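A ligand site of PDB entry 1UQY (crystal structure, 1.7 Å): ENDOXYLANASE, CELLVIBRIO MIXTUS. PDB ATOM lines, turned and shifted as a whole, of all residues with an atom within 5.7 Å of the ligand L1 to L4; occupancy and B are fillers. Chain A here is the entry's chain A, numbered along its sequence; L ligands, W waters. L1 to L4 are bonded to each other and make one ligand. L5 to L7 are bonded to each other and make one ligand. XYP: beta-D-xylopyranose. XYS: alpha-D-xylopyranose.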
ATOM      1  N   TRP A 108      24.457   3.129 -22.883  1.00  0.00           N
ATOM      2  CA  TRP A 108      23.186   2.634 -23.359  1.00  0.00           C
ATOM      3  C   TRP A 108      23.334   2.229 -24.819  1.00  0.00           C
ATOM      4  O   TRP A 108      24.161   2.765 -25.547  1.00  0.00           O
ATOM      5  CB  TRP A 108      22.151   3.745 -23.190  1.00  0.00           C
ATOM      6  CG  TRP A 108      20.746   3.387 -23.448  1.00  0.00           C
ATOM      7  CD1 TRP A 108      20.115   2.174 -23.221  1.00  0.00           C
ATOM      8  CD2 TRP A 108      19.729   4.274 -23.912  1.00  0.00           C
ATOM      9  NE1 TRP A 108      18.779   2.294 -23.522  1.00  0.00           N
ATOM     10  CE2 TRP A 108      18.518   3.566 -23.966  1.00  0.00           C
ATOM     11  CE3 TRP A 108      19.736   5.618 -24.329  1.00  0.00           C
ATOM     12  CZ2 TRP A 108      17.292   4.167 -24.362  1.00  0.00           C
ATOM     13  CZ3 TRP A 108      18.533   6.203 -24.762  1.00  0.00           C
ATOM     14  CH2 TRP A 108      17.336   5.472 -24.772  1.00  0.00           C
ATOM     15  N   SER A 110      20.946   2.518 -27.192  1.00  0.00           N
ATOM     16  CA  SER A 110      20.078   3.334 -28.029  1.00  0.00           C
ATOM     17  C   SER A 110      20.584   4.778 -28.149  1.00  0.00           C
ATOM     18  O   SER A 110      21.273   5.258 -27.238  1.00  0.00           O
ATOM     19  CB  SER A 110      18.660   3.323 -27.441  1.00  0.00           C
ATOM     20  OG  SER A 110      17.704   3.751 -28.382  1.00  0.00           O
ATOM     21  N   ASN A 156      21.845   1.824 -18.736  1.00  0.00           N
ATOM     22  CA  ASN A 156      20.359   1.788 -19.031  1.00  0.00           C
ATOM     23  C   ASN A 156      20.125   0.484 -19.817  1.00  0.00           C
ATOM     24  O   ASN A 156      20.861   0.194 -20.763  1.00  0.00           O
ATOM     25  CB  ASN A 156      19.946   2.978 -19.934  1.00  0.00           C
ATOM     26  CG  ASN A 156      18.506   3.496 -19.722  1.00  0.00           C
ATOM     27  OD1 ASN A 156      17.962   3.415 -18.626  1.00  0.00           O
ATOM     28  ND2 ASN A 156      17.894   4.063 -20.789  1.00  0.00           N
ATOM     29  N   GLU A 157      19.144  -0.321 -19.379  1.00  0.00           N
ATOM     30  CA  GLU A 157      18.500  -1.319 -20.247  1.00  0.00           C
ATOM     31  C   GLU A 157      19.433  -2.442 -20.713  1.00  0.00           C
ATOM     32  O   GLU A 157      19.495  -2.794 -21.911  1.00  0.00           O
ATOM     33  CB  GLU A 157      17.822  -0.609 -21.410  1.00  0.00           C
ATOM     34  CG  GLU A 157      16.711   0.355 -21.003  1.00  0.00           C
ATOM     35  CD  GLU A 157      16.039   1.079 -22.149  1.00  0.00           C
ATOM     36  OE1 GLU A 157      16.335   0.767 -23.326  1.00  0.00           O
ATOM     37  OE2 GLU A 157      15.203   1.961 -21.861  1.00  0.00           O
ATOM     38  N   ASP A 161      14.558  -8.385 -23.067  1.00  0.00           N
ATOM     39  CA  ASP A 161      13.206  -8.775 -22.696  1.00  0.00           C
ATOM     40  C   ASP A 161      12.938 -10.254 -22.726  1.00  0.00           C
ATOM     41  O   ASP A 161      11.940 -10.698 -22.172  1.00  0.00           O
ATOM     42  CB  ASP A 161      12.239  -8.014 -23.518  1.00  0.00           C
ATOM     43  CG  ASP A 161      12.171  -6.551 -23.102  1.00  0.00           C
ATOM     44  OD1 ASP A 161      11.887  -6.213 -21.891  1.00  0.00           O
ATOM     45  OD2 ASP A 161      12.278  -5.698 -23.995  1.00  0.00           O
ATOM     46  N   TYR A 200      13.392  -0.659 -17.894  1.00  0.00           N
ATOM     47  CA  TYR A 200      11.932  -0.729 -18.042  1.00  0.00           C
ATOM     48  C   TYR A 200      11.458  -2.177 -17.894  1.00  0.00           C
ATOM     49  O   TYR A 200      12.208  -3.142 -18.177  1.00  0.00           O
ATOM     50  CB  TYR A 200      11.472  -0.157 -19.414  1.00  0.00           C
ATOM     51  CG  TYR A 200      11.896  -1.001 -20.599  1.00  0.00           C
ATOM     52  CD1 TYR A 200      11.106  -2.042 -21.075  1.00  0.00           C
ATOM     53  CD2 TYR A 200      13.107  -0.776 -21.234  1.00  0.00           C
ATOM     54  CE1 TYR A 200      11.498  -2.820 -22.160  1.00  0.00           C
ATOM     55  CE2 TYR A 200      13.502  -1.526 -22.318  1.00  0.00           C
ATOM     56  CZ  TYR A 200      12.714  -2.561 -22.771  1.00  0.00           C
ATOM     57  OH  TYR A 200      13.168  -3.310 -23.839  1.00  0.00           O
ATOM     58  N   ASN A 201      10.201  -2.321 -17.477  1.00  0.00           N
ATOM     59  CA  ASN A 201       9.560  -3.638 -17.336  1.00  0.00           C
ATOM     60  C   ASN A 201      10.163  -4.461 -16.207  1.00  0.00           C
ATOM     61  O   ASN A 201       9.847  -5.633 -16.056  1.00  0.00           O
ATOM     62  CB  ASN A 201       9.519  -4.411 -18.664  1.00  0.00           C
ATOM     63  CG  ASN A 201       8.417  -3.968 -19.586  1.00  0.00           C
ATOM     64  OD1 ASN A 201       7.534  -3.162 -19.201  1.00  0.00           O
ATOM     65  ND2 ASN A 201       8.440  -4.485 -20.842  1.00  0.00           N
ATOM     66  N   ARG A 204       7.953  -6.148 -13.474  1.00  0.00           N
ATOM     67  CA  ARG A 204       7.270  -7.410 -13.760  1.00  0.00           C
ATOM     68  C   ARG A 204       8.074  -8.635 -13.425  1.00  0.00           C
ATOM     69  O   ARG A 204       9.298  -8.657 -13.526  1.00  0.00           O
ATOM     70  CB  ARG A 204       6.931  -7.459 -15.256  1.00  0.00           C
ATOM     71  CG  ARG A 204       5.847  -6.480 -15.718  1.00  0.00           C
ATOM     72  CD  ARG A 204       5.900  -6.249 -17.227  1.00  0.00           C
ATOM     73  NE  ARG A 204       4.935  -5.246 -17.711  1.00  0.00           N
ATOM     74  CZ  ARG A 204       3.632  -5.507 -17.984  1.00  0.00           C
ATOM     75  NH1 ARG A 204       3.128  -6.726 -17.777  1.00  0.00           N
ATOM     76  NH2 ARG A 204       2.835  -4.536 -18.433  1.00  0.00           N
ATOM     77  N   GLN A 231      11.887   2.425 -14.501  1.00  0.00           N
ATOM     78  CA  GLN A 231      11.417   3.479 -15.409  1.00  0.00           C
ATOM     79  C   GLN A 231       9.976   3.846 -15.125  1.00  0.00           C
ATOM     80  O   GLN A 231       9.658   5.028 -15.059  1.00  0.00           O
ATOM     81  CB  GLN A 231      11.661   3.135 -16.878  1.00  0.00           C
ATOM     82  CG  GLN A 231      13.124   3.258 -17.246  1.00  0.00           C
ATOM     83  CD  GLN A 231      13.372   2.978 -18.707  1.00  0.00           C
ATOM     84  OE1 GLN A 231      12.449   3.009 -19.513  1.00  0.00           O
ATOM     85  NE2 GLN A 231      14.635   2.637 -19.053  1.00  0.00           N
ATOM     86  N   HIS A 233       7.236   3.145 -17.062  1.00  0.00           N
ATOM     87  CA  HIS A 233       6.414   3.380 -18.266  1.00  0.00           C
ATOM     88  C   HIS A 233       5.226   2.446 -18.163  1.00  0.00           C
ATOM     89  O   HIS A 233       5.326   1.285 -18.549  1.00  0.00           O
ATOM     90  CB  HIS A 233       7.220   3.097 -19.525  1.00  0.00           C
ATOM     91  CG  HIS A 233       8.250   4.150 -19.798  1.00  0.00           C
ATOM     92  ND1 HIS A 233       7.940   5.483 -19.876  1.00  0.00           N
ATOM     93  CD2 HIS A 233       9.591   4.046 -19.974  1.00  0.00           C
ATOM     94  CE1 HIS A 233       9.046   6.173 -20.112  1.00  0.00           C
ATOM     95  NE2 HIS A 233      10.067   5.331 -20.171  1.00  0.00           N
ATOM     96  N   LEU A 234       4.154   2.919 -17.578  1.00  0.00           N
ATOM     97  CA  LEU A 234       3.013   2.082 -17.239  1.00  0.00           C
ATOM     98  C   LEU A 234       1.890   2.202 -18.253  1.00  0.00           C
ATOM     99  O   LEU A 234       1.800   3.171 -18.997  1.00  0.00           O
ATOM    100  CB  LEU A 234       2.435   2.483 -15.893  1.00  0.00           C
ATOM    101  CG  LEU A 234       3.340   2.588 -14.671  1.00  0.00           C
ATOM    102  CD1 LEU A 234       2.445   3.103 -13.504  1.00  0.00           C
ATOM    103  CD2 LEU A 234       4.037   1.275 -14.391  1.00  0.00           C
ATOM    104  N   ASP A 237      -3.922   0.119 -17.320  1.00  0.00           N
ATOM    105  CA  ASP A 237      -4.264  -1.043 -16.490  1.00  0.00           C
ATOM    106  C   ASP A 237      -3.069  -1.822 -15.928  1.00  0.00           C
ATOM    107  O   ASP A 237      -3.019  -2.114 -14.727  1.00  0.00           O
ATOM    108  CB  ASP A 237      -5.189  -1.994 -17.263  1.00  0.00           C
ATOM    109  CG  ASP A 237      -6.498  -1.349 -17.654  1.00  0.00           C
ATOM    110  OD1 ASP A 237      -7.208  -0.862 -16.748  1.00  0.00           O
ATOM    111  OD2 ASP A 237      -6.886  -1.286 -18.853  1.00  0.00           O
ATOM    112  N   THR A 238      -2.092  -2.138 -16.779  1.00  0.00           N
ATOM    113  CA  THR A 238      -0.990  -3.052 -16.456  1.00  0.00           C
ATOM    114  C   THR A 238       0.299  -2.253 -16.358  1.00  0.00           C
ATOM    115  O   THR A 238       0.443  -1.230 -17.050  1.00  0.00           O
ATOM    116  CB  THR A 238      -0.770  -4.075 -17.610  1.00  0.00           C
ATOM    117  OG1 THR A 238      -0.517  -3.372 -18.838  1.00  0.00           O
ATOM    118  CG2 THR A 238      -2.034  -4.924 -17.842  1.00  0.00           C
ATOM    119  N   SER A 270      -3.346  -0.421 -26.970  1.00  0.00           N
ATOM    120  CA  SER A 270      -2.054  -1.036 -26.913  1.00  0.00           C
ATOM    121  C   SER A 270      -1.840  -1.994 -28.063  1.00  0.00           C
ATOM    122  O   SER A 270      -2.740  -2.792 -28.412  1.00  0.00           O
ATOM    123  CB  SER A 270      -1.934  -1.821 -25.615  1.00  0.00           C
ATOM    124  OG  SER A 270      -0.662  -2.434 -25.534  1.00  0.00           O
ATOM    125  N   VAL A 271      -0.637  -1.926 -28.637  1.00  0.00           N
ATOM    126  CA  VAL A 271      -0.266  -2.816 -29.728  1.00  0.00           C
ATOM    127  C   VAL A 271       0.849  -3.783 -29.315  1.00  0.00           C
ATOM    128  O   VAL A 271       1.391  -4.497 -30.130  1.00  0.00           O
ATOM    129  CB  VAL A 271       0.111  -1.991 -30.962  1.00  0.00           C
ATOM    130  CG1 VAL A 271      -1.057  -1.103 -31.425  1.00  0.00           C
ATOM    131  CG2 VAL A 271       1.351  -1.154 -30.725  1.00  0.00           C
ATOM    132  N   TRP A 272       1.186  -3.836 -28.037  1.00  0.00           N
ATOM    133  CA  TRP A 272       2.326  -4.635 -27.587  1.00  0.00           C
ATOM    134  C   TRP A 272       2.111  -6.125 -27.726  1.00  0.00           C
ATOM    135  O   TRP A 272       3.062  -6.840 -28.041  1.00  0.00           O
ATOM    136  CB  TRP A 272       2.722  -4.277 -26.151  1.00  0.00           C
ATOM    137  CG  TRP A 272       3.238  -2.888 -26.061  1.00  0.00           C
ATOM    138  CD1 TRP A 272       2.680  -1.844 -25.364  1.00  0.00           C
ATOM    139  CD2 TRP A 272       4.393  -2.352 -26.716  1.00  0.00           C
ATOM    140  NE1 TRP A 272       3.427  -0.707 -25.551  1.00  0.00           N
ATOM    141  CE2 TRP A 272       4.496  -0.991 -26.352  1.00  0.00           C
ATOM    142  CE3 TRP A 272       5.379  -2.897 -27.544  1.00  0.00           C
ATOM    143  CZ2 TRP A 272       5.522  -0.154 -26.813  1.00  0.00           C
ATOM    144  CZ3 TRP A 272       6.411  -2.068 -27.994  1.00  0.00           C
ATOM    145  CH2 TRP A 272       6.480  -0.718 -27.629  1.00  0.00           C
ATOM    146  N   GLU A 273       0.880  -6.594 -27.550  1.00  0.00           N
ATOM    147  CA  GLU A 273       0.631  -8.040 -27.565  1.00  0.00           C
ATOM    148  C   GLU A 273      -0.379  -8.521 -28.623  1.00  0.00           C
ATOM    149  O   GLU A 273      -1.214  -9.380 -28.354  1.00  0.00           O
ATOM    150  CB  GLU A 273       0.216  -8.474 -26.178  1.00  0.00           C
ATOM    151  CG  GLU A 273       1.328  -8.237 -25.175  1.00  0.00           C
ATOM    152  CD  GLU A 273       1.065  -8.869 -23.846  1.00  0.00           C
ATOM    153  OE1 GLU A 273      -0.126  -9.154 -23.529  1.00  0.00           O
ATOM    154  OE2 GLU A 273       2.058  -9.063 -23.101  1.00  0.00           O
ATOM    155  N   TRP A 336       6.847  11.698 -25.076  1.00  0.00           N
ATOM    156  CA  TRP A 336       7.347  10.823 -26.132  1.00  0.00           C
ATOM    157  C   TRP A 336       6.299   9.779 -26.587  1.00  0.00           C
ATOM    158  O   TRP A 336       6.441   9.210 -27.636  1.00  0.00           O
ATOM    159  CB  TRP A 336       8.617  10.095 -25.664  1.00  0.00           C
ATOM    160  CG  TRP A 336       8.392   8.974 -24.652  1.00  0.00           C
ATOM    161  CD1 TRP A 336       7.741   9.065 -23.427  1.00  0.00           C
ATOM    162  CD2 TRP A 336       8.811   7.633 -24.775  1.00  0.00           C
ATOM    163  NE1 TRP A 336       7.709   7.841 -22.832  1.00  0.00           N
ATOM    164  CE2 TRP A 336       8.384   6.943 -23.623  1.00  0.00           C
ATOM    165  CE3 TRP A 336       9.495   6.909 -25.763  1.00  0.00           C
ATOM    166  CZ2 TRP A 336       8.622   5.585 -23.421  1.00  0.00           C
ATOM    167  CZ3 TRP A 336       9.756   5.549 -25.537  1.00  0.00           C
ATOM    168  CH2 TRP A 336       9.312   4.909 -24.385  1.00  0.00           C
ATOM    169  N   PHE A 340       5.511   7.307 -29.819  1.00  0.00           N
ATOM    170  CA  PHE A 340       5.998   5.995 -29.582  1.00  0.00           C
ATOM    171  C   PHE A 340       4.916   5.223 -28.849  1.00  0.00           C
ATOM    172  O   PHE A 340       4.388   5.747 -27.873  1.00  0.00           O
ATOM    173  CB  PHE A 340       7.259   6.042 -28.707  1.00  0.00           C
ATOM    174  CG  PHE A 340       7.803   4.673 -28.409  1.00  0.00           C
ATOM    175  CD1 PHE A 340       8.659   4.043 -29.287  1.00  0.00           C
ATOM    176  CD2 PHE A 340       7.424   4.013 -27.262  1.00  0.00           C
ATOM    177  CE1 PHE A 340       9.128   2.746 -28.997  1.00  0.00           C
ATOM    178  CE2 PHE A 340       7.890   2.731 -26.988  1.00  0.00           C
ATOM    179  CZ  PHE A 340       8.731   2.123 -27.849  1.00  0.00           C
HETATM  180  O1  XYP L   1      -4.079  -4.996 -21.637  1.00  0.00           O
HETATM  181  C1  XYP L   1      -2.891  -5.597 -22.113  1.00  0.00           C
HETATM  182  C2  XYP L   1      -2.501  -5.034 -23.452  1.00  0.00           C
HETATM  183  C3  XYP L   1      -1.097  -5.488 -23.832  1.00  0.00           C
HETATM  184  C4  XYP L   1      -0.118  -5.190 -22.692  1.00  0.00           C
HETATM  185  C5  XYP L   1      -0.654  -5.900 -21.460  1.00  0.00           C
HETATM  186  O2  XYP L   1      -3.376  -5.494 -24.465  1.00  0.00           O
HETATM  187  O3  XYP L   1      -0.754  -4.901 -25.075  1.00  0.00           O
HETATM  188  O4  XYP L   1       1.169  -5.713 -22.956  1.00  0.00           O
HETATM  189  O5  XYP L   1      -1.939  -5.371 -21.172  1.00  0.00           O
HETATM  190  C1  XYP L   2       2.262  -4.954 -22.365  1.00  0.00           C
HETATM  191  C2  XYP L   2       3.552  -5.698 -22.616  1.00  0.00           C
HETATM  192  C3  XYP L   2       4.785  -4.915 -22.130  1.00  0.00           C
HETATM  193  C4  XYP L   2       4.701  -3.509 -22.683  1.00  0.00           C
HETATM  194  C5  XYP L   2       3.355  -2.934 -22.252  1.00  0.00           C
HETATM  195  O2  XYP L   2       3.531  -6.960 -21.948  1.00  0.00           O
HETATM  196  O3  XYP L   2       5.990  -5.519 -22.538  1.00  0.00           O
HETATM  197  O4  XYP L   2       5.732  -2.736 -22.123  1.00  0.00           O
HETATM  198  O5  XYP L   2       2.289  -3.675 -22.826  1.00  0.00           O
HETATM  199  C1  XYP L   3       6.426  -1.933 -23.098  1.00  0.00           C
HETATM  200  C2  XYP L   3       6.714  -0.626 -22.420  1.00  0.00           C
HETATM  201  C3  XYP L   3       7.552   0.253 -23.302  1.00  0.00           C
HETATM  202  C4  XYP L   3       8.813  -0.478 -23.694  1.00  0.00           C
HETATM  203  C5  XYP L   3       8.469  -1.839 -24.272  1.00  0.00           C
HETATM  204  O2  XYP L   3       5.516   0.065 -22.116  1.00  0.00           O
HETATM  205  O3  XYP L   3       7.849   1.439 -22.625  1.00  0.00           O
HETATM  206  O4  XYP L   3       9.451   0.309 -24.668  1.00  0.00           O
HETATM  207  O5  XYP L   3       7.574  -2.561 -23.452  1.00  0.00           O
HETATM  208  C1  XYP L   4      10.688   0.807 -24.190  1.00  0.00           C
HETATM  209  C2  XYP L   4      11.457   1.216 -25.409  1.00  0.00           C
HETATM  210  C3  XYP L   4      12.796   1.770 -25.037  1.00  0.00           C
HETATM  211  C4  XYP L   4      12.561   2.912 -24.088  1.00  0.00           C
HETATM  212  C5  XYP L   4      11.779   2.384 -22.894  1.00  0.00           C
HETATM  213  O2  XYP L   4      11.637   0.099 -26.266  1.00  0.00           O
HETATM  214  O3  XYP L   4      13.396   2.188 -26.238  1.00  0.00           O
HETATM  215  O4  XYP L   4      13.775   3.549 -23.704  1.00  0.00           O
HETATM  216  O5  XYP L   4      10.525   1.851 -23.340  1.00  0.00           O
HETATM  217  C1  XYS L   5      13.214   5.358 -21.400  1.00  0.00           C
HETATM  218  C2  XYS L   5      14.605   5.892 -21.720  1.00  0.00           C
HETATM  219  C3  XYS L   5      14.531   7.324 -22.209  1.00  0.00           C
HETATM  220  C4  XYS L   5      13.600   7.350 -23.412  1.00  0.00           C
HETATM  221  C5  XYS L   5      12.232   6.917 -22.956  1.00  0.00           C
HETATM  222  O1  XYS L   5      12.728   5.945 -20.212  1.00  0.00           O
HETATM  223  O2  XYS L   5      15.380   5.748 -20.537  1.00  0.00           O
HETATM  224  O3  XYS L   5      15.850   7.781 -22.586  1.00  0.00           O
HETATM  225  O4  XYS L   5      13.508   8.703 -23.793  1.00  0.00           O
HETATM  226  O5  XYS L   5      12.309   5.639 -22.348  1.00  0.00           O
HETATM  227  C1  XYP L   6      13.076   8.902 -25.148  1.00  0.00           C
HETATM  228  C2  XYP L   6      12.795  10.384 -25.315  1.00  0.00           C
HETATM  229  C3  XYP L   6      12.449  10.703 -26.745  1.00  0.00           C
HETATM  230  C4  XYP L   6      13.489  10.098 -27.672  1.00  0.00           C
HETATM  231  C5  XYP L   6      13.698   8.641 -27.313  1.00  0.00           C
HETATM  232  O2  XYP L   6      11.755  10.799 -24.467  1.00  0.00           O
HETATM  233  O3  XYP L   6      12.295  12.095 -26.930  1.00  0.00           O
HETATM  234  O4  XYP L   6      12.947  10.186 -28.969  1.00  0.00           O
HETATM  235  O5  XYP L   6      14.084   8.504 -25.963  1.00  0.00           O
HETATM  236  C1  XYP L   7      13.909  10.436 -29.982  1.00  0.00           C
HETATM  237  C2  XYP L   7      13.232  10.019 -31.268  1.00  0.00           C
HETATM  238  C3  XYP L   7      14.203  10.185 -32.411  1.00  0.00           C
HETATM  239  C4  XYP L   7      14.707  11.620 -32.418  1.00  0.00           C
HETATM  240  C5  XYP L   7      15.263  11.970 -31.033  1.00  0.00           C
HETATM  241  O2  XYP L   7      12.949   8.639 -31.230  1.00  0.00           O
HETATM  242  O3  XYP L   7      13.553   9.820 -33.612  1.00  0.00           O
HETATM  243  O4  XYP L   7      15.724  11.700 -33.398  1.00  0.00           O
HETATM  244  O5  XYP L   7      14.320  11.731 -29.983  1.00  0.00           O
HETATM  245  O   HOH W   1      -1.956  -5.426 -27.534  1.00  0.00           O
HETATM  246  O   HOH W   2      -5.386  -5.913 -18.956  1.00  0.00           O
HETATM  247  O   HOH W   3       9.743  -4.002 -26.315  1.00  0.00           O
HETATM  248  O   HOH W   4       5.783  -5.812 -25.298  1.00  0.00           O
HETATM  249  O   HOH W   5       4.859   2.748 -22.505  1.00  0.00           O
HETATM  250  O   HOH W   6       7.546  -0.356 -19.166  1.00  0.00           O
HETATM  251  O   HOH W   7       8.807  -5.266 -24.159  1.00  0.00           O
HETATM  252  O   HOH W   8      13.739   4.997 -26.249  1.00  0.00           O
HETATM  253  O   HOH W   9      13.582  -1.777 -26.189  1.00  0.00           O
HETATM  254  O   HOH W  10      15.932   1.335 -25.868  1.00  0.00           O
HETATM  255  O   HOH W  11       8.086  -8.087 -22.738  1.00  0.00           O
HETATM  256  O   HOH W  12       3.774  -0.447 -20.089  1.00  0.00           O
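Residues that only touch the ligand L1 to L4: Trp 272 (3.2 Å), Trp 336 (3.5 Å), Gln 231 (3.5 Å), His 233 (3.6 Å), Trp 108 (3.6 Å), Phe 340 (3.7 Å), Tyr 200 (3.8 Å) and Arg 204 (3.995 Å).
Hydrophobic or aromatic side chains that line the ligand L1 to L4: Trp 108, Tyr 200, His 233, Trp 272, Trp 336 and Phe 340.
The nearest printed residue that does not touch the ligand L1 to L4 is Val 271 (4.6 Å).
O5 of XYS L5 sits at hydrogen-bond distance from O4 of XYP L4, 2.9 Å away.
Water W10 bridges OE1 of Glu 157 (2.6 Å) and O3 of XYP L4 (2.7 Å).
Water W9 bridges an oxygen (O2) of XYP L4 (2.7 Å) and the side-chain hydroxyl of Tyr 200 (2.8 Å).
Water W12 bridges an oxygen (O2) of XYP L3 (2.7 Å) and the backbone carbonyl oxygen of His 233 (2.8 Å).
Water W1 lies within hydrogen-bond range of O3 of XYP L1 (2.8 Å), O of Ser 270 (2.9 Å) and N of Glu 273 (3.1 Å).
Water W7 bridges O5 of XYP L3 and ND2 of Asn 201.
Water W6 lies within hydrogen-bond range of the side-chain amide oxygen of Asn 201 (2.8 Å) and the backbone carbonyl oxygen of His 233 (2.8 Å).
O5 of XYP L1 lies close to OG1 of Thr 238 (3.4 Å).
The side-chain hydroxyl (OG) of Ser 270 is in hydrogen-bond range of an oxygen (O3) of XYP L1, 2.5 Å away.
An oxygen (O4) of XYP L4 sits at hydrogen-bond distance from the side-chain carboxylate of Glu 157, at 2.8 Å.
A ring nitrogen (NE2) of His 233 lies within hydrogen-bond range of an oxygen (O1) of XYS L5.
O1 of XYS L5 lies within hydrogen-bond range of OE1 of Gln 231, at 3.0 Å.
ND2 of Asn 156 sits at hydrogen-bond distance from O2 of XYS L5 (3.0 Å).
O2 of XYP L2 is in hydrogen-bond range of OE2 of Glu 273, at 2.8 Å.
The backbone NH (N) of Glu 273 sits at hydrogen-bond distance from an oxygen (O3) of XYP L1 (3.4 Å).
The side-chain amide nitrogen (ND2) of Asn 201 is in hydrogen-bond range of an oxygen (O3) of XYP L2, at 3.2 Å.
The side-chain amide nitrogen (NE2) of Gln 231 sits at hydrogen-bond distance from the side-chain amide oxygen (OD1) of Asn 156 (3.4 Å).
The side-chain hydroxyl (OH) of Tyr 200 sits at hydrogen-bond distance from the side-chain carboxylate (OD2) of Asp 161, 2.6 Å away.
OG of Ser 270 sits close to N of Trp 272 (3.4 Å).
The indole nitrogen of Trp 108 sits close to the side-chain amide nitrogen of Asn 156 (3.4 Å).
The side-chain carboxylate of Glu 157 lies within hydrogen-bond range of the side-chain amide nitrogen of Gln 231 (2.9 Å).
OE1 of Glu 157 is in hydrogen-bond range of NE1 of Trp 108 (2.9 Å).
A ring nitrogen (NE2) of His 233 lies close to the side-chain amide oxygen of Gln 231.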
